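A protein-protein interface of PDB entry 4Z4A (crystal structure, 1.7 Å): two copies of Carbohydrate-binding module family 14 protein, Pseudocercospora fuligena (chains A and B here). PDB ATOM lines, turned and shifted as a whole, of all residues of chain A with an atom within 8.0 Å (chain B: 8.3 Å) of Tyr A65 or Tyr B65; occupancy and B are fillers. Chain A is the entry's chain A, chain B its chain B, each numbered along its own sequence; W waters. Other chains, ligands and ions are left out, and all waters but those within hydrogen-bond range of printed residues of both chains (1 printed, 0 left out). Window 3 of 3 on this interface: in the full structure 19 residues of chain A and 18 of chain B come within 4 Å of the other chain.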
ATOM      1  N   PRO A  29      12.800 -13.348  19.229  1.00  0.00           N
ATOM      2  CA  PRO A  29      11.565 -14.123  19.121  1.00  0.00           C
ATOM      3  C   PRO A  29      10.364 -13.290  18.661  1.00  0.00           C
ATOM      4  O   PRO A  29       9.971 -12.341  19.323  1.00  0.00           O
ATOM      5  CB  PRO A  29      11.349 -14.673  20.530  1.00  0.00           C
ATOM      6  CG  PRO A  29      12.740 -14.718  21.111  1.00  0.00           C
ATOM      7  CD  PRO A  29      13.418 -13.479  20.578  1.00  0.00           C
ATOM      8  N   ALA A  30       9.820 -13.658  17.501  1.00  0.00           N
ATOM      9  CA  ALA A  30       8.688 -12.965  16.908  1.00  0.00           C
ATOM     10  C   ALA A  30       7.526 -12.827  17.876  1.00  0.00           C
ATOM     11  O   ALA A  30       6.887 -11.793  17.896  1.00  0.00           O
ATOM     12  CB  ALA A  30       8.210 -13.676  15.645  1.00  0.00           C
ATOM     13  N   ALA A  31       7.263 -13.875  18.673  1.00  0.00           N
ATOM     14  CA  ALA A  31       6.117 -13.850  19.574  1.00  0.00           C
ATOM     15  C   ALA A  31       6.260 -12.794  20.651  1.00  0.00           C
ATOM     16  O   ALA A  31       5.301 -12.178  21.063  1.00  0.00           O
ATOM     17  CB  ALA A  31       5.908 -15.220  20.202  1.00  0.00           C
ATOM     18  N   ASP A  32       7.478 -12.584  21.123  1.00  0.00           N
ATOM     19  CA  ASP A  32       7.718 -11.553  22.156  1.00  0.00           C
ATOM     20  C   ASP A  32       7.511 -10.157  21.572  1.00  0.00           C
ATOM     21  O   ASP A  32       6.946  -9.284  22.199  1.00  0.00           O
ATOM     22  CB  ASP A  32       9.144 -11.655  22.706  1.00  0.00           C
ATOM     23  CG  ASP A  32       9.361 -12.885  23.569  1.00  0.00           C
ATOM     24  OD1 ASP A  32       8.380 -13.567  23.912  1.00  0.00           O
ATOM     25  OD2 ASP A  32      10.526 -13.189  23.852  1.00  0.00           O
ATOM     26  N   ILE A  33       7.975  -9.938  20.361  1.00  0.00           N
ATOM     27  CA  ILE A  33       7.810  -8.630  19.748  1.00  0.00           C
ATOM     28  C   ILE A  33       6.340  -8.341  19.456  1.00  0.00           C
ATOM     29  O   ILE A  33       5.842  -7.254  19.716  1.00  0.00           O
ATOM     30  CB  ILE A  33       8.648  -8.487  18.474  1.00  0.00           C
ATOM     31  CG1 ILE A  33      10.150  -8.678  18.774  1.00  0.00           C
ATOM     32  CG2 ILE A  33       8.479  -7.082  17.897  1.00  0.00           C
ATOM     33  CD1 ILE A  33      10.948  -8.893  17.501  1.00  0.00           C
ATOM     34  N   LYS A  34       5.661  -9.340  18.904  1.00  0.00           N
ATOM     35  CA  LYS A  34       4.278  -9.196  18.479  1.00  0.00           C
ATOM     36  C   LYS A  34       3.402  -8.961  19.686  1.00  0.00           C
ATOM     37  O   LYS A  34       2.536  -8.097  19.653  1.00  0.00           O
ATOM     38  CB  LYS A  34       3.823 -10.460  17.746  1.00  0.00           C
ATOM     39  CG  LYS A  34       2.342 -10.483  17.344  1.00  0.00           C
ATOM     40  CD  LYS A  34       1.855  -9.207  16.678  1.00  0.00           C
ATOM     41  CE  LYS A  34       2.540  -8.918  15.352  1.00  0.00           C
ATOM     42  NZ  LYS A  34       1.708  -7.979  14.528  1.00  0.00           N
ATOM     43  N   THR A  35       3.635  -9.710  20.750  1.00  0.00           N
ATOM     44  CA  THR A  35       2.765  -9.626  21.924  1.00  0.00           C
ATOM     45  C   THR A  35       2.992  -8.411  22.783  1.00  0.00           C
ATOM     46  O   THR A  35       2.027  -7.840  23.285  1.00  0.00           O
ATOM     47  CB  THR A  35       2.785 -10.916  22.803  1.00  0.00           C
ATOM     48  OG1 THR A  35       4.070 -11.096  23.397  1.00  0.00           O
ATOM     49  CG2 THR A  35       2.444 -12.117  21.995  1.00  0.00           C
ATOM     50  N   THR A  36       4.236  -7.948  22.903  1.00  0.00           N
ATOM     51  CA  THR A  36       4.549  -6.827  23.787  1.00  0.00           C
ATOM     52  C   THR A  36       4.859  -5.511  23.074  1.00  0.00           C
ATOM     53  O   THR A  36       4.829  -4.466  23.713  1.00  0.00           O
ATOM     54  CB  THR A  36       5.760  -7.146  24.683  1.00  0.00           C
ATOM     55  OG1 THR A  36       6.959  -7.149  23.901  1.00  0.00           O
ATOM     56  CG2 THR A  36       5.589  -8.512  25.403  1.00  0.00           C
ATOM     57  N   LYS A  37       5.168  -5.573  21.777  1.00  0.00           N
ATOM     58  CA  LYS A  37       5.700  -4.429  21.033  1.00  0.00           C
ATOM     59  C   LYS A  37       6.948  -3.859  21.701  1.00  0.00           C
ATOM     60  O   LYS A  37       7.363  -2.724  21.423  1.00  0.00           O
ATOM     61  CB  LYS A  37       4.611  -3.379  20.762  1.00  0.00           C
ATOM     62  CG  LYS A  37       3.488  -3.954  19.892  1.00  0.00           C
ATOM     63  CD  LYS A  37       2.614  -2.866  19.277  1.00  0.00           C
ATOM     64  CE  LYS A  37       1.613  -3.444  18.280  1.00  0.00           C
ATOM     65  NZ  LYS A  37       0.518  -4.081  19.036  1.00  0.00           N
ATOM     66  N   CYS A  38       7.594  -4.688  22.540  1.00  0.00           N
ATOM     67  CA  CYS A  38       8.732  -4.257  23.343  1.00  0.00           C
ATOM     68  C   CYS A  38       8.502  -2.983  24.152  1.00  0.00           C
ATOM     69  O   CYS A  38       9.432  -2.209  24.390  1.00  0.00           O
ATOM     70  CB  CYS A  38       9.964  -4.120  22.436  1.00  0.00           C
ATOM     71  SG  CYS A  38      10.334  -5.640  21.517  1.00  0.00           S
ATOM     72  N   LEU A  39       7.268  -2.750  24.596  1.00  0.00           N
ATOM     73  CA  LEU A  39       6.943  -1.488  25.220  1.00  0.00           C
ATOM     74  C   LEU A  39       7.413  -1.382  26.659  1.00  0.00           C
ATOM     75  O   LEU A  39       7.846  -0.317  27.100  1.00  0.00           O
ATOM     76  CB  LEU A  39       5.431  -1.179  25.154  1.00  0.00           C
ATOM     77  CG  LEU A  39       4.842  -0.963  23.775  1.00  0.00           C
ATOM     78  CD1 LEU A  39       3.327  -0.782  23.861  1.00  0.00           C
ATOM     79  CD2 LEU A  39       5.473   0.236  23.100  1.00  0.00           C
ATOM     80  N   SER A  59      14.586  -4.337  19.543  1.00  0.00           N
ATOM     81  CA  SER A  59      13.613  -3.258  19.255  1.00  0.00           C
ATOM     82  C   SER A  59      12.879  -3.667  17.976  1.00  0.00           C
ATOM     83  O   SER A  59      13.487  -4.256  17.090  1.00  0.00           O
ATOM     84  CB  SER A  59      14.304  -1.863  19.115  1.00  0.00           C
ATOM     85  OG  SER A  59      15.169  -1.721  18.009  1.00  0.00           O
ATOM     86  N   PRO A  60      11.563  -3.407  17.899  1.00  0.00           N
ATOM     87  CA  PRO A  60      10.803  -3.726  16.653  1.00  0.00           C
ATOM     88  C   PRO A  60      11.441  -3.096  15.431  1.00  0.00           C
ATOM     89  O   PRO A  60      11.710  -1.869  15.399  1.00  0.00           O
ATOM     90  CB  PRO A  60       9.405  -3.123  16.911  1.00  0.00           C
ATOM     91  CG  PRO A  60       9.336  -3.013  18.396  1.00  0.00           C
ATOM     92  CD  PRO A  60      10.726  -2.707  18.875  1.00  0.00           C
ATOM     93  N   ALA A  61      11.629  -3.898  14.394  1.00  0.00           N
ATOM     94  CA  ALA A  61      12.366  -3.462  13.208  1.00  0.00           C
ATOM     95  C   ALA A  61      11.404  -2.657  12.242  1.00  0.00           C
ATOM     96  O   ALA A  61      11.848  -1.716  11.575  1.00  0.00           O
ATOM     97  CB  ALA A  61      12.951  -4.639  12.491  1.00  0.00           C
ATOM     98  N   ASP A  62      10.118  -3.002  12.289  1.00  0.00           N
ATOM     99  CA  ASP A  62       9.099  -2.308  11.462  1.00  0.00           C
ATOM    100  C   ASP A  62       7.705  -2.459  12.068  1.00  0.00           C
ATOM    101  O   ASP A  62       7.534  -3.039  13.130  1.00  0.00           O
ATOM    102  CB  ASP A  62       9.185  -2.832  10.031  1.00  0.00           C
ATOM    103  CG  ASP A  62       8.880  -4.309   9.914  1.00  0.00           C
ATOM    104  OD1 ASP A  62       7.984  -4.810  10.616  1.00  0.00           O
ATOM    105  OD2 ASP A  62       9.456  -4.969   9.013  1.00  0.00           O
ATOM    106  N   ASP A  63       6.683  -1.902  11.421  1.00  0.00           N
ATOM    107  CA  ASP A  63       5.372  -1.885  12.023  1.00  0.00           C
ATOM    108  C   ASP A  63       4.620  -3.198  11.960  1.00  0.00           C
ATOM    109  O   ASP A  63       3.473  -3.266  12.379  1.00  0.00           O
ATOM    110  CB  ASP A  63       4.528  -0.713  11.469  1.00  0.00           C
ATOM    111  CG  ASP A  63       4.317  -0.769   9.979  1.00  0.00           C
ATOM    112  OD1 ASP A  63       4.649  -1.773   9.321  1.00  0.00           O
ATOM    113  OD2 ASP A  63       3.766   0.223   9.431  1.00  0.00           O
ATOM    114  N   SER A  64       5.255  -4.268  11.483  1.00  0.00           N
ATOM    115  CA  SER A  64       4.649  -5.590  11.569  1.00  0.00           C
ATOM    116  C   SER A  64       4.849  -6.162  12.970  1.00  0.00           C
ATOM    117  O   SER A  64       4.144  -7.082  13.399  1.00  0.00           O
ATOM    118  CB  SER A  64       5.223  -6.532  10.517  1.00  0.00           C
ATOM    119  OG  SER A  64       6.475  -7.044  10.987  1.00  0.00           O
ATOM    120  N   TYR A  65       5.818  -5.605  13.682  1.00  0.00           N
ATOM    121  CA  TYR A  65       6.141  -6.096  15.042  1.00  0.00           C
ATOM    122  C   TYR A  65       6.404  -7.619  15.117  1.00  0.00           C
ATOM    123  O   TYR A  65       6.113  -8.294  16.117  1.00  0.00           O
ATOM    124  CB  TYR A  65       5.067  -5.665  16.025  1.00  0.00           C
ATOM    125  CG  TYR A  65       5.027  -4.170  16.239  1.00  0.00           C
ATOM    126  CD1 TYR A  65       5.864  -3.546  17.133  1.00  0.00           C
ATOM    127  CD2 TYR A  65       4.121  -3.374  15.539  1.00  0.00           C
ATOM    128  CE1 TYR A  65       5.816  -2.156  17.317  1.00  0.00           C
ATOM    129  CE2 TYR A  65       4.056  -2.007  15.718  1.00  0.00           C
ATOM    130  CZ  TYR A  65       4.912  -1.384  16.582  1.00  0.00           C
ATOM    131  OH  TYR A  65       4.850  -0.010  16.785  1.00  0.00           O
ATOM    132  N   LEU A  66       7.023  -8.146  14.087  1.00  0.00           N
ATOM    133  CA  LEU A  66       7.376  -9.560  14.057  1.00  0.00           C
ATOM    134  C   LEU A  66       8.870  -9.791  14.041  1.00  0.00           C
ATOM    135  O   LEU A  66       9.313 -10.934  14.172  1.00  0.00           O
ATOM    136  CB  LEU A  66       6.809 -10.207  12.808  1.00  0.00           C
ATOM    137  CG  LEU A  66       5.298 -10.373  12.741  1.00  0.00           C
ATOM    138  CD1 LEU A  66       4.970 -10.984  11.381  1.00  0.00           C
ATOM    139  CD2 LEU A  66       4.819 -11.266  13.873  1.00  0.00           C
ATOM    140  N   THR A  67       9.665  -8.734  13.848  1.00  0.00           N
ATOM    141  CA  THR A  67      11.098  -8.867  13.709  1.00  0.00           C
ATOM    142  C   THR A  67      11.810  -7.791  14.536  1.00  0.00           C
ATOM    143  O   THR A  67      11.230  -6.754  14.871  1.00  0.00           O
ATOM    144  CB  THR A  67      11.607  -8.798  12.251  1.00  0.00           C
ATOM    145  OG1 THR A  67      11.238  -7.554  11.631  1.00  0.00           O
ATOM    146  CG2 THR A  67      11.033  -9.897  11.386  1.00  0.00           C
ATOM    147  N   GLY A  68      13.068  -8.061  14.875  1.00  0.00           N
ATOM    148  CA  GLY A  68      13.785  -7.156  15.746  1.00  0.00           C
ATOM    149  C   GLY A  68      15.173  -6.761  15.305  1.00  0.00           C
ATOM    150  O   GLY A  68      15.919  -7.559  14.769  1.00  0.00           O
ATOM    151  N   ALA B  30       6.050  13.797  27.033  1.00  0.00           N
ATOM    152  CA  ALA B  30       5.502  13.280  25.796  1.00  0.00           C
ATOM    153  C   ALA B  30       6.424  13.497  24.611  1.00  0.00           C
ATOM    154  O   ALA B  30       6.368  12.754  23.641  1.00  0.00           O
ATOM    155  CB  ALA B  30       4.154  13.943  25.497  1.00  0.00           C
ATOM    156  N   ALA B  31       7.224  14.559  24.648  1.00  0.00           N
ATOM    157  CA  ALA B  31       8.080  14.863  23.533  1.00  0.00           C
ATOM    158  C   ALA B  31       9.007  13.688  23.242  1.00  0.00           C
ATOM    159  O   ALA B  31       9.284  13.379  22.091  1.00  0.00           O
ATOM    160  CB  ALA B  31       8.888  16.090  23.805  1.00  0.00           C
ATOM    161  N   ASP B  32       9.518  13.046  24.291  1.00  0.00           N
ATOM    162  CA  ASP B  32      10.453  11.946  24.076  1.00  0.00           C
ATOM    163  C   ASP B  32       9.766  10.707  23.446  1.00  0.00           C
ATOM    164  O   ASP B  32      10.332  10.017  22.595  1.00  0.00           O
ATOM    165  CB  ASP B  32      11.119  11.528  25.378  1.00  0.00           C
ATOM    166  CG  ASP B  32      12.223  12.477  25.834  1.00  0.00           C
ATOM    167  OD1 ASP B  32      12.837  13.152  24.978  1.00  0.00           O
ATOM    168  OD2 ASP B  32      12.529  12.454  27.053  1.00  0.00           O
ATOM    169  N   ILE B  33       8.555  10.433  23.891  1.00  0.00           N
ATOM    170  CA  ILE B  33       7.778   9.319  23.349  1.00  0.00           C
ATOM    171  C   ILE B  33       7.461   9.584  21.903  1.00  0.00           C
ATOM    172  O   ILE B  33       7.608   8.716  21.067  1.00  0.00           O
ATOM    173  CB  ILE B  33       6.510   9.110  24.176  1.00  0.00           C
ATOM    174  CG1 ILE B  33       6.927   8.598  25.569  1.00  0.00           C
ATOM    175  CG2 ILE B  33       5.599   8.061  23.518  1.00  0.00           C
ATOM    176  CD1 ILE B  33       6.184   9.263  26.674  1.00  0.00           C
ATOM    177  N   LYS B  34       7.013  10.797  21.590  1.00  0.00           N
ATOM    178  CA  LYS B  34       6.643  11.098  20.202  1.00  0.00           C
ATOM    179  C   LYS B  34       7.822  11.103  19.258  1.00  0.00           C
ATOM    180  O   LYS B  34       7.707  10.667  18.133  1.00  0.00           O
ATOM    181  CB  LYS B  34       5.937  12.463  20.097  1.00  0.00           C
ATOM    182  CG  LYS B  34       4.591  12.596  20.777  1.00  0.00           C
ATOM    183  CD  LYS B  34       4.212  14.085  20.720  1.00  0.00           C
ATOM    184  CE  LYS B  34       2.729  14.343  20.637  1.00  0.00           C
ATOM    185  NZ  LYS B  34       2.129  14.384  21.996  1.00  0.00           N
ATOM    186  N   THR B  35       8.963  11.609  19.709  1.00  0.00           N
ATOM    187  CA  THR B  35      10.096  11.806  18.860  1.00  0.00           C
ATOM    188  C   THR B  35      10.888  10.519  18.623  1.00  0.00           C
ATOM    189  O   THR B  35      11.412  10.318  17.544  1.00  0.00           O
ATOM    190  CB  THR B  35      11.015  12.874  19.473  1.00  0.00           C
ATOM    191  OG1 THR B  35      10.351  14.142  19.390  1.00  0.00           O
ATOM    192  CG2 THR B  35      12.275  12.986  18.720  1.00  0.00           C
ATOM    193  N   THR B  36      10.963   9.665  19.638  1.00  0.00           N
ATOM    194  CA  THR B  36      11.822   8.443  19.610  1.00  0.00           C
ATOM    195  C   THR B  36      11.043   7.142  19.575  1.00  0.00           C
ATOM    196  O   THR B  36      11.610   6.114  19.173  1.00  0.00           O
ATOM    197  CB  THR B  36      12.776   8.337  20.854  1.00  0.00           C
ATOM    198  OG1 THR B  36      12.041   8.151  22.067  1.00  0.00           O
ATOM    199  CG2 THR B  36      13.684   9.574  20.949  1.00  0.00           C
ATOM    200  N   LYS B  37       9.792   7.176  20.068  1.00  0.00           N
ATOM    201  CA  LYS B  37       8.952   6.000  20.282  1.00  0.00           C
ATOM    202  C   LYS B  37       9.624   5.067  21.307  1.00  0.00           C
ATOM    203  O   LYS B  37       9.285   3.879  21.404  1.00  0.00           O
ATOM    204  CB  LYS B  37       8.669   5.248  18.982  1.00  0.00           C
ATOM    205  CG  LYS B  37       7.805   6.026  18.014  1.00  0.00           C
ATOM    206  CD  LYS B  37       7.411   5.086  16.888  1.00  0.00           C
ATOM    207  CE  LYS B  37       6.319   5.677  16.019  1.00  0.00           C
ATOM    208  NZ  LYS B  37       6.994   6.490  14.996  1.00  0.00           N
ATOM    209  N   CYS B  38      10.571   5.640  22.035  1.00  0.00           N
ATOM    210  CA  CYS B  38      11.390   4.899  22.996  1.00  0.00           C
ATOM    211  C   CYS B  38      12.040   3.640  22.421  1.00  0.00           C
ATOM    212  O   CYS B  38      12.299   2.691  23.162  1.00  0.00           O
ATOM    213  CB  CYS B  38      10.540   4.576  24.235  1.00  0.00           C
ATOM    214  SG  CYS B  38       9.773   5.989  25.080  1.00  0.00           S
ATOM    215  N   LEU B  39      12.324   3.627  21.104  1.00  0.00           N
ATOM    216  CA  LEU B  39      12.808   2.449  20.421  1.00  0.00           C
ATOM    217  C   LEU B  39      14.233   2.113  20.791  1.00  0.00           C
ATOM    218  O   LEU B  39      14.564   0.935  20.885  1.00  0.00           O
ATOM    219  CB  LEU B  39      12.710   2.641  18.891  1.00  0.00           C
ATOM    220  CG  LEU B  39      11.262   2.615  18.436  1.00  0.00           C
ATOM    221  CD1 LEU B  39      11.192   3.000  16.955  1.00  0.00           C
ATOM    222  CD2 LEU B  39      10.632   1.249  18.602  1.00  0.00           C
ATOM    223  N   CYS B  44      14.221   7.304  26.778  1.00  0.00           N
ATOM    224  CA  CYS B  44      13.120   7.301  27.735  1.00  0.00           C
ATOM    225  C   CYS B  44      13.573   6.731  29.090  1.00  0.00           C
ATOM    226  O   CYS B  44      12.789   6.153  29.847  1.00  0.00           O
ATOM    227  CB  CYS B  44      11.934   6.528  27.157  1.00  0.00           C
ATOM    228  SG  CYS B  44      11.383   7.199  25.570  1.00  0.00           S
ATOM    229  N   SER B  59       7.500   4.126  29.471  1.00  0.00           N
ATOM    230  CA  SER B  59       7.081   3.222  28.419  1.00  0.00           C
ATOM    231  C   SER B  59       5.974   3.882  27.618  1.00  0.00           C
ATOM    232  O   SER B  59       5.060   4.451  28.188  1.00  0.00           O
ATOM    233  CB  SER B  59       6.565   1.900  28.996  1.00  0.00           C
ATOM    234  OG  SER B  59       7.618   1.097  29.518  1.00  0.00           O
ATOM    235  N   PRO B  60       6.026   3.797  26.289  1.00  0.00           N
ATOM    236  CA  PRO B  60       4.849   4.350  25.586  1.00  0.00           C
ATOM    237  C   PRO B  60       3.563   3.638  25.985  1.00  0.00           C
ATOM    238  O   PRO B  60       3.613   2.446  26.231  1.00  0.00           O
ATOM    239  CB  PRO B  60       5.134   4.024  24.123  1.00  0.00           C
ATOM    240  CG  PRO B  60       6.646   3.923  24.066  1.00  0.00           C
ATOM    241  CD  PRO B  60       7.011   3.242  25.350  1.00  0.00           C
ATOM    242  N   ALA B  61       2.456   4.387  26.058  1.00  0.00           N
ATOM    243  CA  ALA B  61       1.207   3.814  26.620  1.00  0.00           C
ATOM    244  C   ALA B  61       0.668   2.753  25.692  1.00  0.00           C
ATOM    245  O   ALA B  61       0.105   1.729  26.117  1.00  0.00           O
ATOM    246  CB  ALA B  61       0.183   4.894  26.840  1.00  0.00           C
ATOM    247  N   ASP B  62       0.846   3.018  24.414  1.00  0.00           N
ATOM    248  CA  ASP B  62       0.408   2.126  23.383  1.00  0.00           C
ATOM    249  C   ASP B  62       1.134   2.488  22.100  1.00  0.00           C
ATOM    250  O   ASP B  62       1.985   3.394  22.083  1.00  0.00           O
ATOM    251  CB  ASP B  62      -1.133   2.269  23.228  1.00  0.00           C
ATOM    252  CG  ASP B  62      -1.565   3.703  22.985  1.00  0.00           C
ATOM    253  OD1 ASP B  62      -0.895   4.400  22.186  1.00  0.00           O
ATOM    254  OD2 ASP B  62      -2.596   4.136  23.568  1.00  0.00           O
ATOM    255  N   ASP B  63       0.774   1.811  21.010  1.00  0.00           N
ATOM    256  CA  ASP B  63       1.419   2.025  19.726  1.00  0.00           C
ATOM    257  C   ASP B  63       0.954   3.262  18.934  1.00  0.00           C
ATOM    258  O   ASP B  63       1.291   3.397  17.760  1.00  0.00           O
ATOM    259  CB  ASP B  63       1.357   0.735  18.892  1.00  0.00           C
ATOM    260  CG  ASP B  63      -0.045   0.416  18.364  1.00  0.00           C
ATOM    261  OD1 ASP B  63      -1.048   1.055  18.782  1.00  0.00           O
ATOM    262  OD2 ASP B  63      -0.128  -0.528  17.539  1.00  0.00           O
ATOM    263  N   SER B  64       0.229   4.185  19.578  1.00  0.00           N
ATOM    264  CA  SER B  64       0.067   5.539  19.051  1.00  0.00           C
ATOM    265  C   SER B  64       1.302   6.388  19.400  1.00  0.00           C
ATOM    266  O   SER B  64       1.585   7.396  18.752  1.00  0.00           O
ATOM    267  CB  SER B  64      -1.158   6.202  19.641  1.00  0.00           C
ATOM    268  OG  SER B  64      -2.298   5.417  19.368  1.00  0.00           O
ATOM    269  N   TYR B  65       2.037   5.961  20.425  1.00  0.00           N
ATOM    270  CA  TYR B  65       3.250   6.659  20.871  1.00  0.00           C
ATOM    271  C   TYR B  65       3.002   8.142  21.127  1.00  0.00           C
ATOM    272  O   TYR B  65       3.703   9.000  20.569  1.00  0.00           O
ATOM    273  CB  TYR B  65       4.418   6.469  19.884  1.00  0.00           C
ATOM    274  CG  TYR B  65       4.776   5.019  19.664  1.00  0.00           C
ATOM    275  CD1 TYR B  65       5.628   4.342  20.541  1.00  0.00           C
ATOM    276  CD2 TYR B  65       4.287   4.327  18.569  1.00  0.00           C
ATOM    277  CE1 TYR B  65       5.969   3.023  20.331  1.00  0.00           C
ATOM    278  CE2 TYR B  65       4.619   2.997  18.341  1.00  0.00           C
ATOM    279  CZ  TYR B  65       5.445   2.353  19.235  1.00  0.00           C
ATOM    280  OH  TYR B  65       5.756   1.048  18.995  1.00  0.00           O
ATOM    281  N   LEU B  66       1.998   8.424  21.945  1.00  0.00           N
ATOM    282  CA  LEU B  66       1.635   9.810  22.254  1.00  0.00           C
ATOM    283  C   LEU B  66       1.895  10.183  23.712  1.00  0.00           C
ATOM    284  O   LEU B  66       2.173  11.342  24.008  1.00  0.00           O
ATOM    285  CB  LEU B  66       0.162  10.072  21.927  1.00  0.00           C
ATOM    286  CG  LEU B  66      -0.236   9.936  20.456  1.00  0.00           C
ATOM    287  CD1 LEU B  66      -1.771   9.974  20.364  1.00  0.00           C
ATOM    288  CD2 LEU B  66       0.417  11.023  19.611  1.00  0.00           C
ATOM    289  N   THR B  67       1.802   9.210  24.617  1.00  0.00           N
ATOM    290  CA  THR B  67       1.994   9.485  26.022  1.00  0.00           C
ATOM    291  C   THR B  67       2.726   8.294  26.592  1.00  0.00           C
ATOM    292  O   THR B  67       2.866   7.238  25.931  1.00  0.00           O
ATOM    293  CB  THR B  67       0.680   9.695  26.775  1.00  0.00           C
ATOM    294  OG1 THR B  67      -0.075   8.487  26.684  1.00  0.00           O
ATOM    295  CG2 THR B  67      -0.112  10.889  26.200  1.00  0.00           C
ATOM    296  N   GLY B  68       3.209   8.486  27.810  1.00  0.00           N
ATOM    297  CA  GLY B  68       4.074   7.529  28.450  1.00  0.00           C
ATOM    298  C   GLY B  68       3.553   7.130  29.800  1.00  0.00           C
ATOM    299  O   GLY B  68       2.818   7.898  30.449  1.00  0.00           O
HETATM  300  O   HOH W   1       7.759  -0.374  20.344  1.00  0.00           O
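Pro B60 touches Leu A39 (CB to CD2, 3.9 Å). CD2 of Leu A39 touches CE1 of Tyr B65, at 3.96 Å. CB of Ser A59 touches O of Leu B39, at 3.3 Å. Leu B39 touches Pro A60 (CD2 to CD, 3.97 Å).
Lys A37 touches Asp B63, but with the chains exchanged Asp A63 does not touch Lys B37 (8.0 Å). Leu A39 touches Ser B59, and with the chains exchanged Ser A59 touches Leu B39. Leu A39 touches Pro B60, and with the chains exchanged Pro A60 touches Leu B39. Leu A39 touches Tyr B65, but with the chains exchanged Tyr A65 does not touch Leu B39 (6.0 Å). Positions printed for both chains: 30, 31, 32, 33, 34, 35, 36, 37, 38, 39, 59, 60, 61, 62, 63, 64, 65, 66, 67 and 68. Of the 7 pairs that touch across the chains among the printed residues, 5 have their exchanged pair printed and touching as well.
Tyr A65 touches just one residue of chain B: Tyr B65 (2.6 Å). Of chain A, only Leu A39 and Tyr A65 come within 4 Å of Tyr B65. Ser A64 touches none of the printed residues of chain B. Of the printed residues of chain B, Leu A39 touches Ser B59, Pro B60 and Tyr B65. Of the printed residues of chain B, Pro A60 touches Leu B39. Of the printed residues of chain B, Lys A37 touches Asp B63 (3.5 Å). Cys A38 touches none of the printed residues of chain B. The nearest residue of chain B that does not touch Tyr A65 is Asp B63 (4.1 Å). The nearest residue of chain A that does not touch Tyr B65 is Lys A37 (4.8 Å).
Water W1 bridges O of Lys A37 (2.6 Å) and OH of Tyr B65 (2.8 Å).
The backbone NH of Lys A34 is in hydrogen-bond range of the backbone carbonyl oxygen of Tyr A65 (3.0 Å). The side-chain sulfur (SG) of Cys B44 is disulfide-bonded to the side-chain sulfur (SG) of Cys B38, at 2.1 Å.
Hydrophobic or aromatic side chains of chain B within 4 Å of the printed part of chain A: Leu B39, Pro B60 and Tyr B65. Printed residues of chain A that touch a printed residue of chain B: Lys A37, Leu A39, Ser A59, Pro A60 and Tyr A65. Hydrophobic or aromatic side chains of chain A that line the printed part of chain B: Leu A39, Pro A60 and Tyr A65.
The side-chain amino group of Lys A37 is in salt-bridge range of the side-chain carboxylate of Asp B63 (3.9 Å). The side-chain hydroxyl (OG) of Ser B59 sits at hydrogen-bond distance from the backbone carbonyl oxygen (O) of Leu A39, 2.8 Å away. The side-chain hydroxyl of Tyr A65 sits at hydrogen-bond distance from the side-chain hydroxyl of Tyr B65, 2.6 Å away.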
